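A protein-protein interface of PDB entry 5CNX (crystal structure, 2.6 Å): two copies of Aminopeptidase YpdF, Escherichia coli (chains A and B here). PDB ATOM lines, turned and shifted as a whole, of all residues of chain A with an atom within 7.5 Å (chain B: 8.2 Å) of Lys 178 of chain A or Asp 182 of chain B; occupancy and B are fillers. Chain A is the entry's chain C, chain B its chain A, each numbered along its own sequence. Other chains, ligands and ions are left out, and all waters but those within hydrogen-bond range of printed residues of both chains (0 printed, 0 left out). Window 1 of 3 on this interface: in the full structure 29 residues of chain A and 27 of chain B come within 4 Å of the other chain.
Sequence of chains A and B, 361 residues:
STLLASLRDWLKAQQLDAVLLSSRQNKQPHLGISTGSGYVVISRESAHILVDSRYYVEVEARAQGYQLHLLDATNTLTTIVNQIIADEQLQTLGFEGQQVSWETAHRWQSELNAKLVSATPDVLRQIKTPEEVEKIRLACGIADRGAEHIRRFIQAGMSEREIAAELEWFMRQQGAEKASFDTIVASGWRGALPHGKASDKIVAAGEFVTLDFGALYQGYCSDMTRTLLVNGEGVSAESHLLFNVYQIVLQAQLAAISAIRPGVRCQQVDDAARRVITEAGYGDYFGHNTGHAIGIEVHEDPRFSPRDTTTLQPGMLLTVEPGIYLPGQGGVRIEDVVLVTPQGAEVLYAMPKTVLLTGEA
The backbone carbonyl oxygen (O) of Met 171 of chain A is in hydrogen-bond range of the backbone NH (N) of Ala 176 of chain A, 3.1 Å away.
The backbone NH (N) of Leu 216 of chain A sits at hydrogen-bond distance from the backbone carbonyl oxygen (O) of Lys 178 of chain A (2.8 Å).
OD2 of Asp 182 of chain B is in salt-bridge range of NZ of Lys 197 of chain B, at 2.5 Å.
The backbone NH (N) of Gln 218 of chain A lies within hydrogen-bond range of the side-chain carboxylate (OE1) of Glu 177 of chain A (2.8 Å).
The backbone NH of Glu 177 of chain A sits at hydrogen-bond distance from the backbone carbonyl oxygen of Leu 216 of chain A (2.7 Å).
The guanidinium group (NE) of Arg 172 of chain A lies within hydrogen-bond range of the backbone carbonyl oxygen (O) of Glu 177 of chain A.
Positions printed for both chains: 168, 179, 180, 181 and 214.
Of the 7 pairs that touch across the chains among the printed residues, none has its exchanged pair printed and touching as well.
Ile 142 of chain A touches none of the printed residues of chain B.
Of the printed residues of chain B, Arg 172 of chain A touches Arg 161, Ala 164 and Glu 168.
Printed residues of chain B within 4 Å of Glu 177 of chain A: Arg 161 (3.6 Å).
Of the printed residues of chain B, Lys 178 of chain A touches Asp 182.
No residue of chain B comes within 4 Å of Ala 179 of chain A.
Of the printed residues of chain A, Ala 164 of chain B touches Arg 172.
Printed residues of chain A within 4 Å of Glu 168 of chain B: Arg 172 (2.6 Å).
Asp 182 of chain B touches just one residue of chain A: Lys 178.
Gly 196 of chain B touches none of the printed residues of chain A.
The nearest residue of chain B that does not touch Lys 178 of chain A is Lys 197 of chain B (5.4 Å).
Hydrophobic or aromatic side chains of chain B within 4 Å of the printed part of chain A: Ala 164.
Along chain B the printed residues that touch a printed residue of chain A span positions 161 to 182.
Printed residues of chain A that touch a printed residue of chain B: Arg 172, Gly 175, Ala 176, Glu 177 and Lys 178.
Among the printed residues, Asp or Glu carboxylates within 4 Å of a Lys or Arg side-chain nitrogen of the other chain: Arg 172 of chain A with Glu 168 of chain B (2.6 Å) and Lys 178 of chain A with Asp 182 of chain B (2.8 Å).
Among the printed residues, merely in contact across the chains: Arg 172 of chain A with Arg 161 of chain B (3.5 Å), Arg 172 of chain A with Ala 164 of chain B (3.7 Å) and Glu 177 of chain A with Arg 161 of chain B (3.6 Å).
The guanidinium group (NH1) of Arg 161 of chain B sits at hydrogen-bond distance from the backbone carbonyl oxygen (O) of Ala 176 of chain A, at 3.1 Å.
NH1 of Arg 172 of chain A is in salt-bridge range of OE2 of Glu 168 of chain B (2.6 Å).
The guanidinium group (NH1) of Arg 161 of chain B is in hydrogen-bond range of the backbone carbonyl oxygen (O) of Gly 175 of chain A (3.4 Å).
The side-chain carboxylate (OD1) of Asp 182 of chain B lies within salt-bridge range of the side-chain amino group (NZ) of Lys 178 of chain A (2.8 Å).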
ATOM      1  N   SER A  34       9.497 -11.708  -5.502  1.00  0.00           N
ATOM      2  CA  SER A  34      10.866 -11.856  -5.972  1.00  0.00           C
ATOM      3  C   SER A  34      11.774 -11.058  -5.046  1.00  0.00           C
ATOM      4  O   SER A  34      11.765  -9.827  -5.066  1.00  0.00           O
ATOM      5  CB  SER A  34      10.997 -11.382  -7.425  1.00  0.00           C
ATOM      6  OG  SER A  34      12.316 -11.541  -7.918  1.00  0.00           O
ATOM      7  N   ILE A 142       0.455  -7.035 -22.374  1.00  0.00           N
ATOM      8  CA  ILE A 142       0.744  -5.690 -21.891  1.00  0.00           C
ATOM      9  C   ILE A 142       1.774  -5.004 -22.779  1.00  0.00           C
ATOM     10  O   ILE A 142       1.639  -3.821 -23.114  1.00  0.00           O
ATOM     11  CB  ILE A 142       1.249  -5.711 -20.436  1.00  0.00           C
ATOM     12  CG1 ILE A 142       0.096  -6.025 -19.482  1.00  0.00           C
ATOM     13  CG2 ILE A 142       1.862  -4.376 -20.057  1.00  0.00           C
ATOM     14  CD1 ILE A 142       0.526  -6.266 -18.044  1.00  0.00           C
ATOM     15  N   GLU A 168       6.884   2.897 -20.437  1.00  0.00           N
ATOM     16  CA  GLU A 168       6.881   2.195 -19.170  1.00  0.00           C
ATOM     17  C   GLU A 168       5.665   2.605 -18.348  1.00  0.00           C
ATOM     18  O   GLU A 168       4.996   1.755 -17.748  1.00  0.00           O
ATOM     19  CB  GLU A 168       8.178   2.458 -18.403  1.00  0.00           C
ATOM     20  CG  GLU A 168       9.355   1.678 -18.966  1.00  0.00           C
ATOM     21  CD  GLU A 168      10.691   2.195 -18.485  1.00  0.00           C
ATOM     22  OE1 GLU A 168      10.727   2.853 -17.417  1.00  0.00           O
ATOM     23  OE2 GLU A 168      11.699   1.971 -19.194  1.00  0.00           O
ATOM     24  N   MET A 171       2.730   0.775 -19.614  1.00  0.00           N
ATOM     25  CA  MET A 171       2.788  -0.632 -19.222  1.00  0.00           C
ATOM     26  C   MET A 171       2.368  -0.808 -17.775  1.00  0.00           C
ATOM     27  O   MET A 171       1.628  -1.734 -17.431  1.00  0.00           O
ATOM     28  CB  MET A 171       4.192  -1.187 -19.412  1.00  0.00           C
ATOM     29  CG  MET A 171       4.625  -1.346 -20.848  1.00  0.00           C
ATOM     30  SD  MET A 171       6.293  -2.025 -20.885  1.00  0.00           S
ATOM     31  CE  MET A 171       5.961  -3.566 -21.717  1.00  0.00           C
ATOM     32  N   ARG A 172       2.854   0.107 -16.943  1.00  0.00           N
ATOM     33  CA  ARG A 172       2.539   0.142 -15.525  1.00  0.00           C
ATOM     34  C   ARG A 172       1.017   0.257 -15.371  1.00  0.00           C
ATOM     35  O   ARG A 172       0.389  -0.564 -14.703  1.00  0.00           O
ATOM     36  CB  ARG A 172       3.274   1.314 -14.867  1.00  0.00           C
ATOM     37  CG  ARG A 172       3.636   1.157 -13.396  1.00  0.00           C
ATOM     38  CD  ARG A 172       4.706   0.116 -13.144  1.00  0.00           C
ATOM     39  NE  ARG A 172       4.339  -0.685 -11.986  1.00  0.00           N
ATOM     40  CZ  ARG A 172       4.679  -0.399 -10.737  1.00  0.00           C
ATOM     41  NH1 ARG A 172       5.436   0.664 -10.481  1.00  0.00           N
ATOM     42  NH2 ARG A 172       4.274  -1.187  -9.750  1.00  0.00           N
ATOM     43  N   GLY A 175      -1.030  -2.812 -15.728  1.00  0.00           N
ATOM     44  CA  GLY A 175      -0.918  -3.838 -14.705  1.00  0.00           C
ATOM     45  C   GLY A 175       0.472  -4.419 -14.509  1.00  0.00           C
ATOM     46  O   GLY A 175       0.685  -5.279 -13.653  1.00  0.00           O
ATOM     47  N   ALA A 176       1.445  -3.915 -15.255  1.00  0.00           N
ATOM     48  CA  ALA A 176       2.805  -4.421 -15.130  1.00  0.00           C
ATOM     49  C   ALA A 176       3.401  -4.022 -13.786  1.00  0.00           C
ATOM     50  O   ALA A 176       3.072  -2.970 -13.238  1.00  0.00           O
ATOM     51  CB  ALA A 176       3.671  -3.905 -16.268  1.00  0.00           C
ATOM     52  N   GLU A 177       4.235  -4.895 -13.233  1.00  0.00           N
ATOM     53  CA  GLU A 177       4.946  -4.597 -12.000  1.00  0.00           C
ATOM     54  C   GLU A 177       6.059  -3.585 -12.266  1.00  0.00           C
ATOM     55  O   GLU A 177       6.416  -2.792 -11.394  1.00  0.00           O
ATOM     56  CB  GLU A 177       5.545  -5.855 -11.400  1.00  0.00           C
ATOM     57  CG  GLU A 177       4.557  -6.845 -10.885  1.00  0.00           C
ATOM     58  CD  GLU A 177       5.244  -8.132 -10.519  1.00  0.00           C
ATOM     59  OE1 GLU A 177       5.476  -8.956 -11.430  1.00  0.00           O
ATOM     60  OE2 GLU A 177       5.593  -8.303  -9.330  1.00  0.00           O
ATOM     61  N   LYS A 178       6.647  -3.699 -13.457  1.00  0.00           N
ATOM     62  CA  LYS A 178       7.685  -2.807 -13.968  1.00  0.00           C
ATOM     63  C   LYS A 178       8.118  -3.320 -15.331  1.00  0.00           C
ATOM     64  O   LYS A 178       7.586  -4.329 -15.813  1.00  0.00           O
ATOM     65  CB  LYS A 178       8.876  -2.726 -13.018  1.00  0.00           C
ATOM     66  CG  LYS A 178       9.517  -4.052 -12.706  1.00  0.00           C
ATOM     67  CD  LYS A 178      10.758  -3.846 -11.882  1.00  0.00           C
ATOM     68  CE  LYS A 178      11.201  -5.132 -11.236  1.00  0.00           C
ATOM     69  NZ  LYS A 178      12.483  -4.932 -10.490  1.00  0.00           N
ATOM     70  N   ALA A 179       9.049  -2.620 -15.974  1.00  0.00           N
ATOM     71  CA  ALA A 179       9.637  -3.139 -17.202  1.00  0.00           C
ATOM     72  C   ALA A 179      10.503  -4.333 -16.815  1.00  0.00           C
ATOM     73  O   ALA A 179      11.071  -4.361 -15.722  1.00  0.00           O
ATOM     74  CB  ALA A 179      10.455  -2.083 -17.926  1.00  0.00           C
ATOM     75  N   SER A 180      10.555  -5.348 -17.670  1.00  0.00           N
ATOM     76  CA  SER A 180      11.353  -6.533 -17.378  1.00  0.00           C
ATOM     77  C   SER A 180      12.862  -6.278 -17.537  1.00  0.00           C
ATOM     78  O   SER A 180      13.679  -7.048 -17.041  1.00  0.00           O
ATOM     79  CB  SER A 180      10.901  -7.686 -18.263  1.00  0.00           C
ATOM     80  OG  SER A 180      10.670  -7.246 -19.582  1.00  0.00           O
ATOM     81  N   PHE A 181      13.228  -5.201 -18.227  1.00  0.00           N
ATOM     82  CA  PHE A 181      14.631  -4.809 -18.351  1.00  0.00           C
ATOM     83  C   PHE A 181      14.677  -3.368 -18.801  1.00  0.00           C
ATOM     84  O   PHE A 181      13.664  -2.853 -19.269  1.00  0.00           O
ATOM     85  CB  PHE A 181      15.378  -5.697 -19.343  1.00  0.00           C
ATOM     86  CG  PHE A 181      14.777  -5.703 -20.714  1.00  0.00           C
ATOM     87  CD1 PHE A 181      13.755  -6.603 -21.036  1.00  0.00           C
ATOM     88  CD2 PHE A 181      15.215  -4.822 -21.679  1.00  0.00           C
ATOM     89  CE1 PHE A 181      13.187  -6.615 -22.296  1.00  0.00           C
ATOM     90  CE2 PHE A 181      14.651  -4.822 -22.946  1.00  0.00           C
ATOM     91  CZ  PHE A 181      13.642  -5.720 -23.261  1.00  0.00           C
ATOM     92  N   GLY A 214       9.919  -4.626 -22.465  1.00  0.00           N
ATOM     93  CA  GLY A 214       9.120  -5.737 -21.987  1.00  0.00           C
ATOM     94  C   GLY A 214       8.483  -5.474 -20.640  1.00  0.00           C
ATOM     95  O   GLY A 214       8.864  -4.548 -19.922  1.00  0.00           O
ATOM     96  N   ALA A 215       7.526  -6.319 -20.275  1.00  0.00           N
ATOM     97  CA  ALA A 215       6.790  -6.127 -19.040  1.00  0.00           C
ATOM     98  C   ALA A 215       7.056  -7.270 -18.095  1.00  0.00           C
ATOM     99  O   ALA A 215       7.229  -8.412 -18.521  1.00  0.00           O
ATOM    100  CB  ALA A 215       5.302  -6.014 -19.312  1.00  0.00           C
ATOM    101  N   LEU A 216       7.129  -6.937 -16.811  1.00  0.00           N
ATOM    102  CA  LEU A 216       7.121  -7.927 -15.747  1.00  0.00           C
ATOM    103  C   LEU A 216       5.706  -7.983 -15.181  1.00  0.00           C
ATOM    104  O   LEU A 216       5.210  -7.010 -14.603  1.00  0.00           O
ATOM    105  CB  LEU A 216       8.129  -7.582 -14.653  1.00  0.00           C
ATOM    106  CG  LEU A 216       8.221  -8.552 -13.466  1.00  0.00           C
ATOM    107  CD1 LEU A 216       8.748  -9.921 -13.896  1.00  0.00           C
ATOM    108  CD2 LEU A 216       9.072  -7.971 -12.356  1.00  0.00           C
ATOM    109  N   TYR A 217       5.051  -9.123 -15.349  1.00  0.00           N
ATOM    110  CA  TYR A 217       3.684  -9.255 -14.897  1.00  0.00           C
ATOM    111  C   TYR A 217       3.618 -10.465 -14.004  1.00  0.00           C
ATOM    112  O   TYR A 217       3.795 -11.593 -14.475  1.00  0.00           O
ATOM    113  CB  TYR A 217       2.732  -9.425 -16.076  1.00  0.00           C
ATOM    114  CG  TYR A 217       1.278  -9.553 -15.680  1.00  0.00           C
ATOM    115  CD1 TYR A 217       0.560  -8.462 -15.216  1.00  0.00           C
ATOM    116  CD2 TYR A 217       0.635 -10.785 -15.729  1.00  0.00           C
ATOM    117  CE1 TYR A 217      -0.770  -8.583 -14.847  1.00  0.00           C
ATOM    118  CE2 TYR A 217      -0.687 -10.917 -15.354  1.00  0.00           C
ATOM    119  CZ  TYR A 217      -1.388  -9.814 -14.918  1.00  0.00           C
ATOM    120  OH  TYR A 217      -2.705  -9.942 -14.540  1.00  0.00           O
ATOM    121  N   GLN A 218       3.365 -10.222 -12.719  1.00  0.00           N
ATOM    122  CA  GLN A 218       3.276 -11.293 -11.741  1.00  0.00           C
ATOM    123  C   GLN A 218       4.480 -12.234 -11.799  1.00  0.00           C
ATOM    124  O   GLN A 218       4.327 -13.457 -11.800  1.00  0.00           O
ATOM    125  CB  GLN A 218       1.977 -12.068 -11.918  1.00  0.00           C
ATOM    126  CG  GLN A 218       0.769 -11.244 -11.541  1.00  0.00           C
ATOM    127  CD  GLN A 218      -0.538 -11.999 -11.702  1.00  0.00           C
ATOM    128  OE1 GLN A 218      -0.627 -12.969 -12.465  1.00  0.00           O
ATOM    129  NE2 GLN A 218      -1.556 -11.576 -10.953  1.00  0.00           N
ATOM    130  N   TYR A 220       6.622 -12.733 -14.231  1.00  0.00           N
ATOM    131  CA  TYR A 220       6.985 -13.289 -15.527  1.00  0.00           C
ATOM    132  C   TYR A 220       7.204 -12.187 -16.555  1.00  0.00           C
ATOM    133  O   TYR A 220       6.644 -11.099 -16.446  1.00  0.00           O
ATOM    134  CB  TYR A 220       5.929 -14.303 -15.986  1.00  0.00           C
ATOM    135  CG  TYR A 220       6.095 -15.614 -15.260  1.00  0.00           C
ATOM    136  CD1 TYR A 220       5.642 -15.772 -13.955  1.00  0.00           C
ATOM    137  CD2 TYR A 220       6.748 -16.679 -15.859  1.00  0.00           C
ATOM    138  CE1 TYR A 220       5.812 -16.965 -13.282  1.00  0.00           C
ATOM    139  CE2 TYR A 220       6.919 -17.877 -15.193  1.00  0.00           C
ATOM    140  CZ  TYR A 220       6.452 -18.013 -13.907  1.00  0.00           C
ATOM    141  OH  TYR A 220       6.635 -19.201 -13.243  1.00  0.00           O
ATOM    142  N   SER A 222       7.940 -10.359 -20.460  1.00  0.00           N
ATOM    143  CA  SER A 222       7.784 -10.320 -21.895  1.00  0.00           C
ATOM    144  C   SER A 222       8.975  -9.536 -22.416  1.00  0.00           C
ATOM    145  O   SER A 222       9.715  -8.926 -21.638  1.00  0.00           O
ATOM    146  CB  SER A 222       6.452  -9.702 -22.322  1.00  0.00           C
ATOM    147  OG  SER A 222       6.291  -8.397 -21.810  1.00  0.00           O
ATOM    148  N   ARG B 161      -0.992   0.489  -7.638  1.00  0.00           N
ATOM    149  CA  ARG B 161      -0.162   0.385  -8.828  1.00  0.00           C
ATOM    150  C   ARG B 161      -0.214   1.681  -9.633  1.00  0.00           C
ATOM    151  O   ARG B 161       0.804   2.161 -10.133  1.00  0.00           O
ATOM    152  CB  ARG B 161      -0.609  -0.796  -9.682  1.00  0.00           C
ATOM    153  CG  ARG B 161       0.248  -1.042 -10.912  1.00  0.00           C
ATOM    154  CD  ARG B 161      -0.238  -2.258 -11.680  1.00  0.00           C
ATOM    155  NE  ARG B 161      -0.524  -3.371 -10.784  1.00  0.00           N
ATOM    156  CZ  ARG B 161       0.389  -4.217 -10.324  1.00  0.00           C
ATOM    157  NH1 ARG B 161       1.655  -4.076 -10.677  1.00  0.00           N
ATOM    158  NH2 ARG B 161       0.038  -5.203  -9.510  1.00  0.00           N
ATOM    159  N   ALA B 164       1.854   4.461  -8.000  1.00  0.00           N
ATOM    160  CA  ALA B 164       3.251   4.205  -8.275  1.00  0.00           C
ATOM    161  C   ALA B 164       3.640   4.660  -9.683  1.00  0.00           C
ATOM    162  O   ALA B 164       4.704   5.260  -9.866  1.00  0.00           O
ATOM    163  CB  ALA B 164       3.560   2.741  -8.089  1.00  0.00           C
ATOM    164  N   GLU B 168       6.621   7.260 -10.341  1.00  0.00           N
ATOM    165  CA  GLU B 168       7.792   6.883 -11.117  1.00  0.00           C
ATOM    166  C   GLU B 168       7.966   7.774 -12.360  1.00  0.00           C
ATOM    167  O   GLU B 168       9.065   8.295 -12.634  1.00  0.00           O
ATOM    168  CB  GLU B 168       7.684   5.418 -11.514  1.00  0.00           C
ATOM    169  CG  GLU B 168       8.050   4.455 -10.395  1.00  0.00           C
ATOM    170  CD  GLU B 168       7.455   3.079 -10.637  1.00  0.00           C
ATOM    171  OE1 GLU B 168       7.085   2.821 -11.805  1.00  0.00           O
ATOM    172  OE2 GLU B 168       7.354   2.267  -9.678  1.00  0.00           O
ATOM    173  N   ALA B 179      13.670   4.460 -11.073  1.00  0.00           N
ATOM    174  CA  ALA B 179      13.524   4.298  -9.639  1.00  0.00           C
ATOM    175  C   ALA B 179      14.712   3.507  -9.141  1.00  0.00           C
ATOM    176  O   ALA B 179      15.184   2.608  -9.827  1.00  0.00           O
ATOM    177  CB  ALA B 179      12.210   3.588  -9.293  1.00  0.00           C
ATOM    178  N   SER B 180      15.208   3.846  -7.961  1.00  0.00           N
ATOM    179  CA  SER B 180      16.360   3.148  -7.424  1.00  0.00           C
ATOM    180  C   SER B 180      15.968   1.768  -6.931  1.00  0.00           C
ATOM    181  O   SER B 180      16.817   0.905  -6.722  1.00  0.00           O
ATOM    182  CB  SER B 180      17.001   3.962  -6.307  1.00  0.00           C
ATOM    183  OG  SER B 180      16.022   4.521  -5.457  1.00  0.00           O
ATOM    184  N   PHE B 181      14.676   1.561  -6.729  1.00  0.00           N
ATOM    185  CA  PHE B 181      14.181   0.243  -6.321  1.00  0.00           C
ATOM    186  C   PHE B 181      12.680   0.165  -6.542  1.00  0.00           C
ATOM    187  O   PHE B 181      12.030   1.188  -6.747  1.00  0.00           O
ATOM    188  CB  PHE B 181      14.516  -0.046  -4.855  1.00  0.00           C
ATOM    189  CG  PHE B 181      13.965   0.969  -3.905  1.00  0.00           C
ATOM    190  CD1 PHE B 181      12.690   0.801  -3.348  1.00  0.00           C
ATOM    191  CD2 PHE B 181      14.700   2.112  -3.588  1.00  0.00           C
ATOM    192  CE1 PHE B 181      12.157   1.734  -2.477  1.00  0.00           C
ATOM    193  CE2 PHE B 181      14.174   3.068  -2.710  1.00  0.00           C
ATOM    194  CZ  PHE B 181      12.892   2.862  -2.144  1.00  0.00           C
ATOM    195  N   ASP B 182      12.142  -1.048  -6.472  1.00  0.00           N
ATOM    196  CA  ASP B 182      10.723  -1.269  -6.700  1.00  0.00           C
ATOM    197  C   ASP B 182       9.897  -0.488  -5.692  1.00  0.00           C
ATOM    198  O   ASP B 182      10.038  -0.674  -4.475  1.00  0.00           O
ATOM    199  CB  ASP B 182      10.386  -2.761  -6.611  1.00  0.00           C
ATOM    200  CG  ASP B 182      11.041  -3.584  -7.724  1.00  0.00           C
ATOM    201  OD1 ASP B 182      11.570  -2.995  -8.687  1.00  0.00           O
ATOM    202  OD2 ASP B 182      11.045  -4.828  -7.630  1.00  0.00           O
ATOM    203  N   THR B 183       9.051   0.401  -6.216  1.00  0.00           N
ATOM    204  CA  THR B 183       8.244   1.303  -5.407  1.00  0.00           C
ATOM    205  C   THR B 183       7.255   0.558  -4.489  1.00  0.00           C
ATOM    206  O   THR B 183       6.536  -0.354  -4.918  1.00  0.00           O
ATOM    207  CB  THR B 183       7.445   2.258  -6.303  1.00  0.00           C
ATOM    208  OG1 THR B 183       8.317   2.857  -7.272  1.00  0.00           O
ATOM    209  CG2 THR B 183       6.764   3.338  -5.483  1.00  0.00           C
ATOM    210  N   ILE B 184       7.232   0.945  -3.217  1.00  0.00           N
ATOM    211  CA  ILE B 184       6.285   0.403  -2.255  1.00  0.00           C
ATOM    212  C   ILE B 184       5.139   1.389  -2.079  1.00  0.00           C
ATOM    213  O   ILE B 184       5.366   2.558  -1.746  1.00  0.00           O
ATOM    214  CB  ILE B 184       6.944   0.150  -0.894  1.00  0.00           C
ATOM    215  CG1 ILE B 184       7.898  -1.044  -0.971  1.00  0.00           C
ATOM    216  CG2 ILE B 184       5.893  -0.061   0.181  1.00  0.00           C
ATOM    217  CD1 ILE B 184       8.831  -1.136   0.214  1.00  0.00           C
ATOM    218  N   VAL B 185       3.917   0.939  -2.345  1.00  0.00           N
ATOM    219  CA  VAL B 185       2.733   1.730  -2.033  1.00  0.00           C
ATOM    220  C   VAL B 185       1.751   0.839  -1.273  1.00  0.00           C
ATOM    221  O   VAL B 185       1.120  -0.029  -1.863  1.00  0.00           O
ATOM    222  CB  VAL B 185       2.073   2.293  -3.309  1.00  0.00           C
ATOM    223  CG1 VAL B 185       0.824   3.090  -2.969  1.00  0.00           C
ATOM    224  CG2 VAL B 185       3.059   3.150  -4.088  1.00  0.00           C
ATOM    225  N   HIS B 195       7.399  -4.190   3.049  1.00  0.00           N
ATOM    226  CA  HIS B 195       7.863  -4.231   1.666  1.00  0.00           C
ATOM    227  C   HIS B 195       6.751  -4.527   0.703  1.00  0.00           C
ATOM    228  O   HIS B 195       6.963  -5.166  -0.325  1.00  0.00           O
ATOM    229  CB  HIS B 195       8.974  -5.252   1.495  1.00  0.00           C
ATOM    230  CG  HIS B 195      10.319  -4.715   1.846  1.00  0.00           C
ATOM    231  ND1 HIS B 195      11.143  -4.122   0.908  1.00  0.00           N
ATOM    232  CD2 HIS B 195      10.961  -4.601   3.035  1.00  0.00           C
ATOM    233  CE1 HIS B 195      12.247  -3.706   1.500  1.00  0.00           C
ATOM    234  NE2 HIS B 195      12.162  -3.979   2.793  1.00  0.00           N
ATOM    235  N   GLY B 196       5.564  -4.052   1.046  1.00  0.00           N
ATOM    236  CA  GLY B 196       4.392  -4.267   0.232  1.00  0.00           C
ATOM    237  C   GLY B 196       4.460  -3.466  -1.048  1.00  0.00           C
ATOM    238  O   GLY B 196       4.008  -2.321  -1.088  1.00  0.00           O
ATOM    239  N   LYS B 197       5.051  -4.054  -2.083  1.00  0.00           N
ATOM    240  CA  LYS B 197       5.115  -3.416  -3.390  1.00  0.00           C
ATOM    241  C   LYS B 197       3.723  -3.068  -3.900  1.00  0.00           C
ATOM    242  O   LYS B 197       2.762  -3.814  -3.664  1.00  0.00           O
ATOM    243  CB  LYS B 197       5.852  -4.316  -4.381  1.00  0.00           C
ATOM    244  CG  LYS B 197       7.328  -4.509  -4.012  1.00  0.00           C
ATOM    245  CD  LYS B 197       8.064  -5.406  -4.992  1.00  0.00           C
ATOM    246  CE  LYS B 197       9.486  -5.649  -4.523  1.00  0.00           C
ATOM    247  NZ  LYS B 197      10.356  -6.105  -5.646  1.00  0.00           N
ATOM    248  N   ALA B 198       3.631  -1.941  -4.610  1.00  0.00           N
ATOM    249  CA  ALA B 198       2.353  -1.416  -5.077  1.00  0.00           C
ATOM    250  C   ALA B 198       1.539  -2.510  -5.771  1.00  0.00           C
ATOM    251  O   ALA B 198       2.032  -3.194  -6.664  1.00  0.00           O
ATOM    252  CB  ALA B 198       2.576  -0.233  -6.015  1.00  0.00           C
ATOM    253  N   ASP B 212       7.075   4.145  -0.167  1.00  0.00           N
ATOM    254  CA  ASP B 212       8.513   3.942  -0.086  1.00  0.00           C
ATOM    255  C   ASP B 212       9.073   3.814  -1.492  1.00  0.00           C
ATOM    256  O   ASP B 212       8.699   2.901  -2.235  1.00  0.00           O
ATOM    257  CB  ASP B 212       8.814   2.695   0.733  1.00  0.00           C
ATOM    258  CG  ASP B 212      10.250   2.615   1.196  1.00  0.00           C
ATOM    259  OD1 ASP B 212      11.149   3.197   0.533  1.00  0.00           O
ATOM    260  OD2 ASP B 212      10.473   1.946   2.231  1.00  0.00           O
ATOM    261  N   PHE B 213       9.987   4.712  -1.841  1.00  0.00           N
ATOM    262  CA  PHE B 213      10.418   4.855  -3.219  1.00  0.00           C
ATOM    263  C   PHE B 213      11.726   5.645  -3.292  1.00  0.00           C
ATOM    264  O   PHE B 213      12.198   6.187  -2.284  1.00  0.00           O
ATOM    265  CB  PHE B 213       9.338   5.559  -4.031  1.00  0.00           C
ATOM    266  CG  PHE B 213       9.106   6.965  -3.591  1.00  0.00           C
ATOM    267  CD1 PHE B 213       8.358   7.230  -2.459  1.00  0.00           C
ATOM    268  CD2 PHE B 213       9.693   8.023  -4.262  1.00  0.00           C
ATOM    269  CE1 PHE B 213       8.167   8.532  -2.032  1.00  0.00           C
ATOM    270  CE2 PHE B 213       9.506   9.312  -3.835  1.00  0.00           C
ATOM    271  CZ  PHE B 213       8.740   9.566  -2.723  1.00  0.00           C
ATOM    272  N   GLY B 214      12.305   5.739  -4.482  1.00  0.00           N
ATOM    273  CA  GLY B 214      13.559   6.449  -4.612  1.00  0.00           C
ATOM    274  C   GLY B 214      13.967   6.631  -6.052  1.00  0.00           C
ATOM    275  O   GLY B 214      13.409   5.995  -6.956  1.00  0.00           O
ATOM    276  N   ASP B 223      16.165   7.502  -1.414  1.00  0.00           N
ATOM    277  CA  ASP B 223      15.318   6.517  -0.760  1.00  0.00           C
ATOM    278  C   ASP B 223      14.408   7.268   0.207  1.00  0.00           C
ATOM    279  O   ASP B 223      14.901   7.821   1.192  1.00  0.00           O
ATOM    280  CB  ASP B 223      16.197   5.491  -0.032  1.00  0.00           C
ATOM    281  CG  ASP B 223      15.423   4.320   0.504  1.00  0.00           C
ATOM    282  OD1 ASP B 223      14.196   4.308   0.329  1.00  0.00           O
ATOM    283  OD2 ASP B 223      16.040   3.408   1.094  1.00  0.00           O
ATOM    284  N   VAL B 298      21.447   1.413  -3.048  1.00  0.00           N
ATOM    285  CA  VAL B 298      20.394   1.773  -2.107  1.00  0.00           C
ATOM    286  C   VAL B 298      20.737   1.305  -0.688  1.00  0.00           C
ATOM    287  O   VAL B 298      20.502   2.037   0.274  1.00  0.00           O
ATOM    288  CB  VAL B 298      19.034   1.201  -2.579  1.00  0.00           C
ATOM    289  CG1 VAL B 298      18.026   1.086  -1.441  1.00  0.00           C
ATOM    290  CG2 VAL B 298      18.492   2.032  -3.735  1.00  0.00           C
